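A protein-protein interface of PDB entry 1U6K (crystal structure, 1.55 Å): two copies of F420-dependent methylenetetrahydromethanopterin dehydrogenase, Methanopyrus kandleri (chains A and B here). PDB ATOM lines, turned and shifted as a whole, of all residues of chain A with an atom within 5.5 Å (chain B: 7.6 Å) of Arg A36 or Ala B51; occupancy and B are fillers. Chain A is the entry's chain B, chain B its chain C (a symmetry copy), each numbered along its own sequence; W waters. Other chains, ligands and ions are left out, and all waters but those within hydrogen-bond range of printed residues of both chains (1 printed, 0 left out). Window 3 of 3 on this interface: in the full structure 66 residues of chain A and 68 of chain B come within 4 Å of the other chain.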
ATOM      1  N   ALA A   6      27.086  19.925  16.691  1.00  0.00           N
ATOM      2  CA  ALA A   6      27.941  20.057  15.525  1.00  0.00           C
ATOM      3  C   ALA A   6      27.156  19.821  14.246  1.00  0.00           C
ATOM      4  O   ALA A   6      26.128  19.142  14.249  1.00  0.00           O
ATOM      5  CB  ALA A   6      29.120  19.070  15.599  1.00  0.00           C
ATOM      6  N   ILE A   7      27.637  20.411  13.168  1.00  0.00           N
ATOM      7  CA  ILE A   7      27.021  20.242  11.870  1.00  0.00           C
ATOM      8  C   ILE A   7      28.062  19.566  10.980  1.00  0.00           C
ATOM      9  O   ILE A   7      29.214  19.982  10.950  1.00  0.00           O
ATOM     10  CB  ILE A   7      26.650  21.581  11.234  1.00  0.00           C
ATOM     11  CG1 ILE A   7      25.587  22.268  12.094  1.00  0.00           C
ATOM     12  CG2 ILE A   7      26.192  21.355   9.804  1.00  0.00           C
ATOM     13  CD1 ILE A   7      25.094  23.573  11.531  1.00  0.00           C
ATOM     14  N   PHE A   8      27.656  18.516  10.271  1.00  0.00           N
ATOM     15  CA  PHE A   8      28.578  17.829   9.370  1.00  0.00           C
ATOM     16  C   PHE A   8      28.137  18.121   7.951  1.00  0.00           C
ATOM     17  O   PHE A   8      26.954  18.007   7.640  1.00  0.00           O
ATOM     18  CB  PHE A   8      28.552  16.308   9.596  1.00  0.00           C
ATOM     19  CG  PHE A   8      29.125  15.876  10.913  1.00  0.00           C
ATOM     20  CD1 PHE A   8      28.353  15.899  12.076  1.00  0.00           C
ATOM     21  CD2 PHE A   8      30.444  15.436  10.998  1.00  0.00           C
ATOM     22  CE1 PHE A   8      28.881  15.494  13.289  1.00  0.00           C
ATOM     23  CE2 PHE A   8      30.986  15.030  12.211  1.00  0.00           C
ATOM     24  CZ  PHE A   8      30.198  15.059  13.368  1.00  0.00           C
ATOM     25  N   GLU A  34      24.274  16.443  19.865  1.00  0.00           N
ATOM     26  CA  GLU A  34      23.174  16.605  18.931  1.00  0.00           C
ATOM     27  C   GLU A  34      23.840  17.003  17.630  1.00  0.00           C
ATOM     28  O   GLU A  34      24.680  17.897  17.624  1.00  0.00           O
ATOM     29  CB  GLU A  34      22.212  17.713  19.353  1.00  0.00           C
ATOM     30  CG  GLU A  34      21.161  17.947  18.277  1.00  0.00           C
ATOM     31  CD  GLU A  34      20.126  18.983  18.653  1.00  0.00           C
ATOM     32  OE1 GLU A  34      19.176  19.174  17.860  1.00  0.00           O
ATOM     33  OE2 GLU A  34      20.260  19.602  19.729  1.00  0.00           O
ATOM     34  N   PHE A  35      23.467  16.354  16.529  1.00  0.00           N
ATOM     35  CA  PHE A  35      24.091  16.646  15.247  1.00  0.00           C
ATOM     36  C   PHE A  35      23.124  16.938  14.122  1.00  0.00           C
ATOM     37  O   PHE A  35      21.970  16.519  14.142  1.00  0.00           O
ATOM     38  CB  PHE A  35      24.942  15.442  14.771  1.00  0.00           C
ATOM     39  CG  PHE A  35      25.991  14.990  15.749  1.00  0.00           C
ATOM     40  CD1 PHE A  35      26.170  13.626  16.012  1.00  0.00           C
ATOM     41  CD2 PHE A  35      26.832  15.907  16.374  1.00  0.00           C
ATOM     42  CE1 PHE A  35      27.170  13.185  16.882  1.00  0.00           C
ATOM     43  CE2 PHE A  35      27.832  15.480  17.243  1.00  0.00           C
ATOM     44  CZ  PHE A  35      28.005  14.110  17.500  1.00  0.00           C
ATOM     45  N   ARG A  36      23.622  17.642  13.118  1.00  0.00           N
ATOM     46  CA  ARG A  36      22.859  17.912  11.905  1.00  0.00           C
ATOM     47  C   ARG A  36      23.814  17.571  10.766  1.00  0.00           C
ATOM     48  O   ARG A  36      24.997  17.872  10.845  1.00  0.00           O
ATOM     49  CB  ARG A  36      22.444  19.379  11.822  1.00  0.00           C
ATOM     50  CG  ARG A  36      21.397  19.762  12.847  1.00  0.00           C
ATOM     51  CD  ARG A  36      20.089  19.034  12.590  1.00  0.00           C
ATOM     52  NE  ARG A  36      19.023  19.588  13.415  1.00  0.00           N
ATOM     53  CZ  ARG A  36      18.892  19.359  14.717  1.00  0.00           C
ATOM     54  NH1 ARG A  36      17.895  19.921  15.391  1.00  0.00           N
ATOM     55  NH2 ARG A  36      19.737  18.551  15.338  1.00  0.00           N
ATOM     56  N   VAL A  37      23.306  16.930   9.722  1.00  0.00           N
ATOM     57  CA  VAL A  37      24.135  16.556   8.587  1.00  0.00           C
ATOM     58  C   VAL A  37      23.508  17.115   7.321  1.00  0.00           C
ATOM     59  O   VAL A  37      22.318  16.961   7.100  1.00  0.00           O
ATOM     60  CB  VAL A  37      24.250  14.999   8.471  1.00  0.00           C
ATOM     61  CG1 VAL A  37      25.223  14.622   7.357  1.00  0.00           C
ATOM     62  CG2 VAL A  37      24.713  14.419   9.786  1.00  0.00           C
ATOM     63  N   VAL A  38      24.312  17.777   6.498  1.00  0.00           N
ATOM     64  CA  VAL A  38      23.826  18.341   5.247  1.00  0.00           C
ATOM     65  C   VAL A  38      24.865  18.183   4.128  1.00  0.00           C
ATOM     66  O   VAL A  38      26.062  18.074   4.395  1.00  0.00           O
ATOM     67  CB  VAL A  38      23.489  19.855   5.398  1.00  0.00           C
ATOM     68  CG1 VAL A  38      22.504  20.053   6.556  1.00  0.00           C
ATOM     69  CG2 VAL A  38      24.764  20.653   5.652  1.00  0.00           C
ATOM     70  N   ILE A  59      21.502  26.952   8.938  1.00  0.00           N
ATOM     71  CA  ILE A  59      20.933  26.270  10.097  1.00  0.00           C
ATOM     72  C   ILE A  59      21.724  26.534  11.385  1.00  0.00           C
ATOM     73  O   ILE A  59      21.195  26.390  12.491  1.00  0.00           O
ATOM     74  CB  ILE A  59      20.837  24.728   9.850  1.00  0.00           C
ATOM     75  CG1 ILE A  59      22.228  24.109   9.851  1.00  0.00           C
ATOM     76  CG2 ILE A  59      20.171  24.443   8.499  1.00  0.00           C
ATOM     77  CD1 ILE A  59      22.220  22.600   9.710  1.00  0.00           C
ATOM     78  N   PHE A  63      20.634  26.585  15.264  1.00  0.00           N
ATOM     79  CA  PHE A  63      21.165  25.376  15.868  1.00  0.00           C
ATOM     80  C   PHE A  63      22.312  25.688  16.811  1.00  0.00           C
ATOM     81  O   PHE A  63      22.456  25.063  17.861  1.00  0.00           O
ATOM     82  CB  PHE A  63      21.619  24.410  14.775  1.00  0.00           C
ATOM     83  CG  PHE A  63      21.985  23.051  15.283  1.00  0.00           C
ATOM     84  CD1 PHE A  63      21.049  22.263  15.940  1.00  0.00           C
ATOM     85  CD2 PHE A  63      23.265  22.544  15.075  1.00  0.00           C
ATOM     86  CE1 PHE A  63      21.378  20.986  16.383  1.00  0.00           C
ATOM     87  CE2 PHE A  63      23.604  21.266  15.515  1.00  0.00           C
ATOM     88  CZ  PHE A  63      22.665  20.486  16.167  1.00  0.00           C
ATOM     89  N   ILE B   9      16.379  12.616   3.097  1.00  0.00           N
ATOM     90  CA  ILE B   9      16.431  12.834   4.537  1.00  0.00           C
ATOM     91  C   ILE B   9      16.881  11.536   5.167  1.00  0.00           C
ATOM     92  O   ILE B   9      16.271  10.487   4.936  1.00  0.00           O
ATOM     93  CB  ILE B   9      15.046  13.189   5.102  1.00  0.00           C
ATOM     94  CG1 ILE B   9      14.416  14.298   4.265  1.00  0.00           C
ATOM     95  CG2 ILE B   9      15.187  13.633   6.552  1.00  0.00           C
ATOM     96  CD1 ILE B   9      12.961  14.597   4.635  1.00  0.00           C
ATOM     97  N   CYS B  11      17.645   9.702   8.806  1.00  0.00           N
ATOM     98  CA  CYS B  11      17.594   9.657  10.269  1.00  0.00           C
ATOM     99  C   CYS B  11      17.745   8.193  10.658  1.00  0.00           C
ATOM    100  O   CYS B  11      16.984   7.336  10.190  1.00  0.00           O
ATOM    101  CB  CYS B  11      16.262  10.198  10.794  1.00  0.00           C
ATOM    102  SG  CYS B  11      15.924  11.917  10.318  1.00  0.00           S
ATOM    103  N   VAL B  38      19.917  15.839   3.893  1.00  0.00           N
ATOM    104  CA  VAL B  38      19.864  16.341   5.258  1.00  0.00           C
ATOM    105  C   VAL B  38      19.438  15.252   6.231  1.00  0.00           C
ATOM    106  O   VAL B  38      18.832  14.252   5.838  1.00  0.00           O
ATOM    107  CB  VAL B  38      18.875  17.548   5.389  1.00  0.00           C
ATOM    108  CG1 VAL B  38      19.376  18.708   4.558  1.00  0.00           C
ATOM    109  CG2 VAL B  38      17.475  17.147   4.933  1.00  0.00           C
ATOM    110  N   GLY B  39      19.749  15.454   7.504  1.00  0.00           N
ATOM    111  CA  GLY B  39      19.378  14.477   8.499  1.00  0.00           C
ATOM    112  C   GLY B  39      19.948  14.791   9.865  1.00  0.00           C
ATOM    113  O   GLY B  39      20.670  15.774  10.045  1.00  0.00           O
ATOM    114  N   THR B  40      19.617  13.943  10.826  1.00  0.00           N
ATOM    115  CA  THR B  40      20.058  14.119  12.195  1.00  0.00           C
ATOM    116  C   THR B  40      20.994  13.009  12.633  1.00  0.00           C
ATOM    117  O   THR B  40      21.069  12.678  13.816  1.00  0.00           O
ATOM    118  CB  THR B  40      18.843  14.148  13.122  1.00  0.00           C
ATOM    119  OG1 THR B  40      18.029  12.997  12.860  1.00  0.00           O
ATOM    120  CG2 THR B  40      18.020  15.409  12.862  1.00  0.00           C
ATOM    121  N   SER B  41      21.704  12.437  11.662  1.00  0.00           N
ATOM    122  CA  SER B  41      22.629  11.356  11.921  1.00  0.00           C
ATOM    123  C   SER B  41      21.836  10.129  12.384  1.00  0.00           C
ATOM    124  O   SER B  41      20.756   9.853  11.853  1.00  0.00           O
ATOM    125  CB  SER B  41      23.668  11.788  12.966  1.00  0.00           C
ATOM    126  OG  SER B  41      24.753  10.874  13.023  1.00  0.00           O
ATOM    127  N   LYS B  43      20.248   9.587  15.254  1.00  0.00           N
ATOM    128  CA  LYS B  43      19.054   9.811  16.055  1.00  0.00           C
ATOM    129  C   LYS B  43      17.802   9.831  15.190  1.00  0.00           C
ATOM    130  O   LYS B  43      17.752  10.505  14.156  1.00  0.00           O
ATOM    131  CB  LYS B  43      19.214  11.104  16.859  1.00  0.00           C
ATOM    132  CG  LYS B  43      20.304  10.967  17.891  1.00  0.00           C
ATOM    133  CD  LYS B  43      20.561  12.237  18.678  1.00  0.00           C
ATOM    134  CE  LYS B  43      21.638  11.980  19.732  1.00  0.00           C
ATOM    135  NZ  LYS B  43      21.387  10.734  20.518  1.00  0.00           N
ATOM    136  N   ASP B  45      14.421   9.759  16.858  1.00  0.00           N
ATOM    137  CA  ASP B  45      13.282   9.928  17.760  1.00  0.00           C
ATOM    138  C   ASP B  45      12.367  10.985  17.139  1.00  0.00           C
ATOM    139  O   ASP B  45      12.765  11.688  16.214  1.00  0.00           O
ATOM    140  CB  ASP B  45      13.755  10.378  19.146  1.00  0.00           C
ATOM    141  CG  ASP B  45      14.647  11.592  19.085  1.00  0.00           C
ATOM    142  OD1 ASP B  45      15.819  11.454  18.665  1.00  0.00           O
ATOM    143  OD2 ASP B  45      14.179  12.694  19.444  1.00  0.00           O
ATOM    144  N   PRO B  46      11.122  11.107  17.634  1.00  0.00           N
ATOM    145  CA  PRO B  46      10.176  12.091  17.096  1.00  0.00           C
ATOM    146  C   PRO B  46      10.709  13.528  16.999  1.00  0.00           C
ATOM    147  O   PRO B  46      10.488  14.204  15.998  1.00  0.00           O
ATOM    148  CB  PRO B  46       8.978  11.963  18.041  1.00  0.00           C
ATOM    149  CG  PRO B  46       8.996  10.502  18.387  1.00  0.00           C
ATOM    150  CD  PRO B  46      10.475  10.254  18.650  1.00  0.00           C
ATOM    151  N   GLU B  47      11.409  13.992  18.030  1.00  0.00           N
ATOM    152  CA  GLU B  47      11.962  15.350  18.017  1.00  0.00           C
ATOM    153  C   GLU B  47      12.951  15.551  16.867  1.00  0.00           C
ATOM    154  O   GLU B  47      12.846  16.504  16.084  1.00  0.00           O
ATOM    155  CB  GLU B  47      12.697  15.642  19.327  1.00  0.00           C
ATOM    156  CG  GLU B  47      11.832  15.648  20.566  1.00  0.00           C
ATOM    157  CD  GLU B  47      12.662  15.663  21.841  1.00  0.00           C
ATOM    158  OE1 GLU B  47      13.285  14.623  22.158  1.00  0.00           O
ATOM    159  OE2 GLU B  47      12.698  16.715  22.519  1.00  0.00           O
ATOM    160  N   CYS B  48      13.922  14.647  16.779  1.00  0.00           N
ATOM    161  CA  CYS B  48      14.944  14.735  15.749  1.00  0.00           C
ATOM    162  C   CYS B  48      14.402  14.579  14.346  1.00  0.00           C
ATOM    163  O   CYS B  48      14.788  15.325  13.459  1.00  0.00           O
ATOM    164  CB  CYS B  48      16.042  13.711  16.017  1.00  0.00           C
ATOM    165  SG  CYS B  48      17.144  14.192  17.378  1.00  0.00           S
ATOM    166  N   VAL B  49      13.513  13.609  14.139  1.00  0.00           N
ATOM    167  CA  VAL B  49      12.939  13.418  12.818  1.00  0.00           C
ATOM    168  C   VAL B  49      12.122  14.639  12.412  1.00  0.00           C
ATOM    169  O   VAL B  49      12.090  15.008  11.243  1.00  0.00           O
ATOM    170  CB  VAL B  49      12.038  12.171  12.762  1.00  0.00           C
ATOM    171  CG1 VAL B  49      11.389  12.053  11.401  1.00  0.00           C
ATOM    172  CG2 VAL B  49      12.869  10.924  13.061  1.00  0.00           C
ATOM    173  N   GLU B  50      11.455  15.283  13.368  1.00  0.00           N
ATOM    174  CA  GLU B  50      10.669  16.461  13.006  1.00  0.00           C
ATOM    175  C   GLU B  50      11.623  17.536  12.525  1.00  0.00           C
ATOM    176  O   GLU B  50      11.416  18.143  11.475  1.00  0.00           O
ATOM    177  CB  GLU B  50       9.847  16.972  14.201  1.00  0.00           C
ATOM    178  CG  GLU B  50       8.877  18.086  13.837  1.00  0.00           C
ATOM    179  CD  GLU B  50       7.913  18.425  14.961  1.00  0.00           C
ATOM    180  OE1 GLU B  50       6.852  19.018  14.670  1.00  0.00           O
ATOM    181  OE2 GLU B  50       8.219  18.106  16.132  1.00  0.00           O
ATOM    182  N   ALA B  51      12.676  17.765  13.295  1.00  0.00           N
ATOM    183  CA  ALA B  51      13.667  18.755  12.917  1.00  0.00           C
ATOM    184  C   ALA B  51      14.221  18.409  11.532  1.00  0.00           C
ATOM    185  O   ALA B  51      14.403  19.289  10.688  1.00  0.00           O
ATOM    186  CB  ALA B  51      14.798  18.789  13.941  1.00  0.00           C
ATOM    187  N   ALA B  52      14.480  17.119  11.299  1.00  0.00           N
ATOM    188  CA  ALA B  52      15.026  16.677  10.015  1.00  0.00           C
ATOM    189  C   ALA B  52      14.115  17.038   8.851  1.00  0.00           C
ATOM    190  O   ALA B  52      14.568  17.604   7.858  1.00  0.00           O
ATOM    191  CB  ALA B  52      15.280  15.148  10.042  1.00  0.00           C
ATOM    192  N   VAL B  53      12.831  16.721   8.973  1.00  0.00           N
ATOM    193  CA  VAL B  53      11.880  17.031   7.910  1.00  0.00           C
ATOM    194  C   VAL B  53      11.667  18.544   7.758  1.00  0.00           C
ATOM    195  O   VAL B  53      11.440  19.034   6.652  1.00  0.00           O
ATOM    196  CB  VAL B  53      10.528  16.344   8.149  1.00  0.00           C
ATOM    197  CG1 VAL B  53       9.633  16.558   6.945  1.00  0.00           C
ATOM    198  CG2 VAL B  53      10.732  14.845   8.366  1.00  0.00           C
ATOM    199  N   GLU B  54      11.759  19.281   8.860  1.00  0.00           N
ATOM    200  CA  GLU B  54      11.606  20.739   8.796  1.00  0.00           C
ATOM    201  C   GLU B  54      12.715  21.311   7.920  1.00  0.00           C
ATOM    202  O   GLU B  54      12.448  22.098   7.002  1.00  0.00           O
ATOM    203  CB  GLU B  54      11.706  21.363  10.182  1.00  0.00           C
ATOM    204  CG  GLU B  54      10.630  20.943  11.162  1.00  0.00           C
ATOM    205  CD  GLU B  54      10.686  21.776  12.430  1.00  0.00           C
ATOM    206  OE1 GLU B  54      10.353  22.978  12.352  1.00  0.00           O
ATOM    207  OE2 GLU B  54      11.078  21.237  13.493  1.00  0.00           O
ATOM    208  N   MET B  55      13.962  20.915   8.209  1.00  0.00           N
ATOM    209  CA  MET B  55      15.129  21.367   7.437  1.00  0.00           C
ATOM    210  C   MET B  55      14.827  21.130   5.965  1.00  0.00           C
ATOM    211  O   MET B  55      14.933  22.035   5.137  1.00  0.00           O
ATOM    212  CB  MET B  55      16.408  20.569   7.785  1.00  0.00           C
ATOM    213  CG  MET B  55      17.104  20.864   9.127  1.00  0.00           C
ATOM    214  SD  MET B  55      18.859  19.932   9.330  1.00  0.00           S
ATOM    215  CE  MET B  55      18.227  18.109   9.187  1.00  0.00           C
ATOM    216  N   ALA B  56      14.455  19.891   5.651  1.00  0.00           N
ATOM    217  CA  ALA B  56      14.144  19.505   4.288  1.00  0.00           C
ATOM    218  C   ALA B  56      13.063  20.382   3.671  1.00  0.00           C
ATOM    219  O   ALA B  56      13.242  20.903   2.570  1.00  0.00           O
ATOM    220  CB  ALA B  56      13.708  18.030   4.246  1.00  0.00           C
ATOM    221  N   LEU B  57      11.942  20.538   4.371  1.00  0.00           N
ATOM    222  CA  LEU B  57      10.844  21.342   3.841  1.00  0.00           C
ATOM    223  C   LEU B  57      11.229  22.811   3.680  1.00  0.00           C
ATOM    224  O   LEU B  57      10.797  23.464   2.739  1.00  0.00           O
ATOM    225  CB  LEU B  57       9.612  21.195   4.731  1.00  0.00           C
ATOM    226  CG  LEU B  57       8.965  19.807   4.601  1.00  0.00           C
ATOM    227  CD1 LEU B  57       7.799  19.684   5.562  1.00  0.00           C
ATOM    228  CD2 LEU B  57       8.497  19.594   3.164  1.00  0.00           C
ATOM    229  N   LYS B  82       6.186  10.016  12.244  1.00  0.00           N
ATOM    230  CA  LYS B  82       6.027  11.466  12.239  1.00  0.00           C
ATOM    231  C   LYS B  82       6.481  12.006  10.882  1.00  0.00           C
ATOM    232  O   LYS B  82       5.875  12.920  10.321  1.00  0.00           O
ATOM    233  CB  LYS B  82       6.853  12.091  13.374  1.00  0.00           C
ATOM    234  CG  LYS B  82       6.566  13.577  13.623  1.00  0.00           C
ATOM    235  CD  LYS B  82       5.119  13.803  14.066  1.00  0.00           C
ATOM    236  CE  LYS B  82       4.868  15.233  14.538  1.00  0.00           C
ATOM    237  NZ  LYS B  82       4.893  16.237  13.440  1.00  0.00           N
ATOM    238  N   MET B  86       4.187  14.118   8.059  1.00  0.00           N
ATOM    239  CA  MET B  86       4.673  15.419   7.585  1.00  0.00           C
ATOM    240  C   MET B  86       4.846  15.461   6.061  1.00  0.00           C
ATOM    241  O   MET B  86       4.458  16.428   5.411  1.00  0.00           O
ATOM    242  CB  MET B  86       5.998  15.782   8.288  1.00  0.00           C
ATOM    243  CG  MET B  86       5.865  15.995   9.800  1.00  0.00           C
ATOM    244  SD  MET B  86       7.485  16.294  10.849  1.00  0.00           S
ATOM    245  CE  MET B  86       7.621  18.234  10.701  1.00  0.00           C
HETATM  246  O   HOH W   1      22.168  13.737  15.931  1.00  0.00           O
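Of the printed residues of chain B, Arg A36 touches Gly B39 (3.6 Å), Ala B51 (3.6 Å) and Met B55 (3.6 Å).
Of chain A, only Arg A36 (3.6 Å) comes within 4 Å of Ala B51.
Of the printed residues of chain B, Phe A35 touches Thr B40.
Of the printed residues of chain A, Thr B40 touches Phe A35.
Of the printed residues of chain B, Val A38 touches Val B38.
Of the printed residues of chain A, Gly B39 touches Arg A36 (3.6 Å) and Val A37 (2.9 Å).
Printed residues of chain A within 4 Å of Met B55: Arg A36 (3.6 Å).
Cys B48 touches none of the printed residues of chain A.
N of Val A37 lies within hydrogen-bond range of O of Gly B39.
Val A38 touches its own counterpart, Val B38.
Position printed for both chains: 38.
O of Phe A8 lies within hydrogen-bond range of N of Val A38.
NH2 of Arg A36 lies within salt-bridge range of OE1 of Glu A34, at 2.7 Å.
The backbone carbonyl oxygen (O) of Lys B43 sits at hydrogen-bond distance from the side-chain hydroxyl (OG1) of Thr B40 (2.8 Å).
SG of Cys B11 sits at hydrogen-bond distance from OG1 of Thr B40.
The backbone NH (N) of Phe A8 lies within hydrogen-bond range of the backbone carbonyl oxygen (O) of Arg A36 (2.8 Å).
The backbone NH (N) of Arg A36 sits at hydrogen-bond distance from the backbone carbonyl oxygen (O) of Ala A6, at 3.1 Å.
Thr B40 touches Phe A35.
Gly B39 touches Arg A36 (O to CA, 3.6 Å).
Arg A36 touches Ala B51.
SD of Met B55 touches CD of Arg A36, at 3.6 Å.
Val B38 touches Val A37.
Val A38 touches Val B38 (CG1 to CG1, 3.9 Å).
Of the 10 printed residues of chain A, 4 touch a printed residue of chain B.
Printed residues of chain A that touch a printed residue of chain B: Phe A35, Arg A36, Val A37 and Val A38.
Among the printed residues, 7 pairs touch across the chains.
Among the printed residues, no Asp or Glu carboxylate lies within 4 Å of a Lys or Arg side-chain nitrogen of the other chain.
Water W1 bridges the backbone carbonyl oxygen of Thr B40 and the backbone NH of Phe A35.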
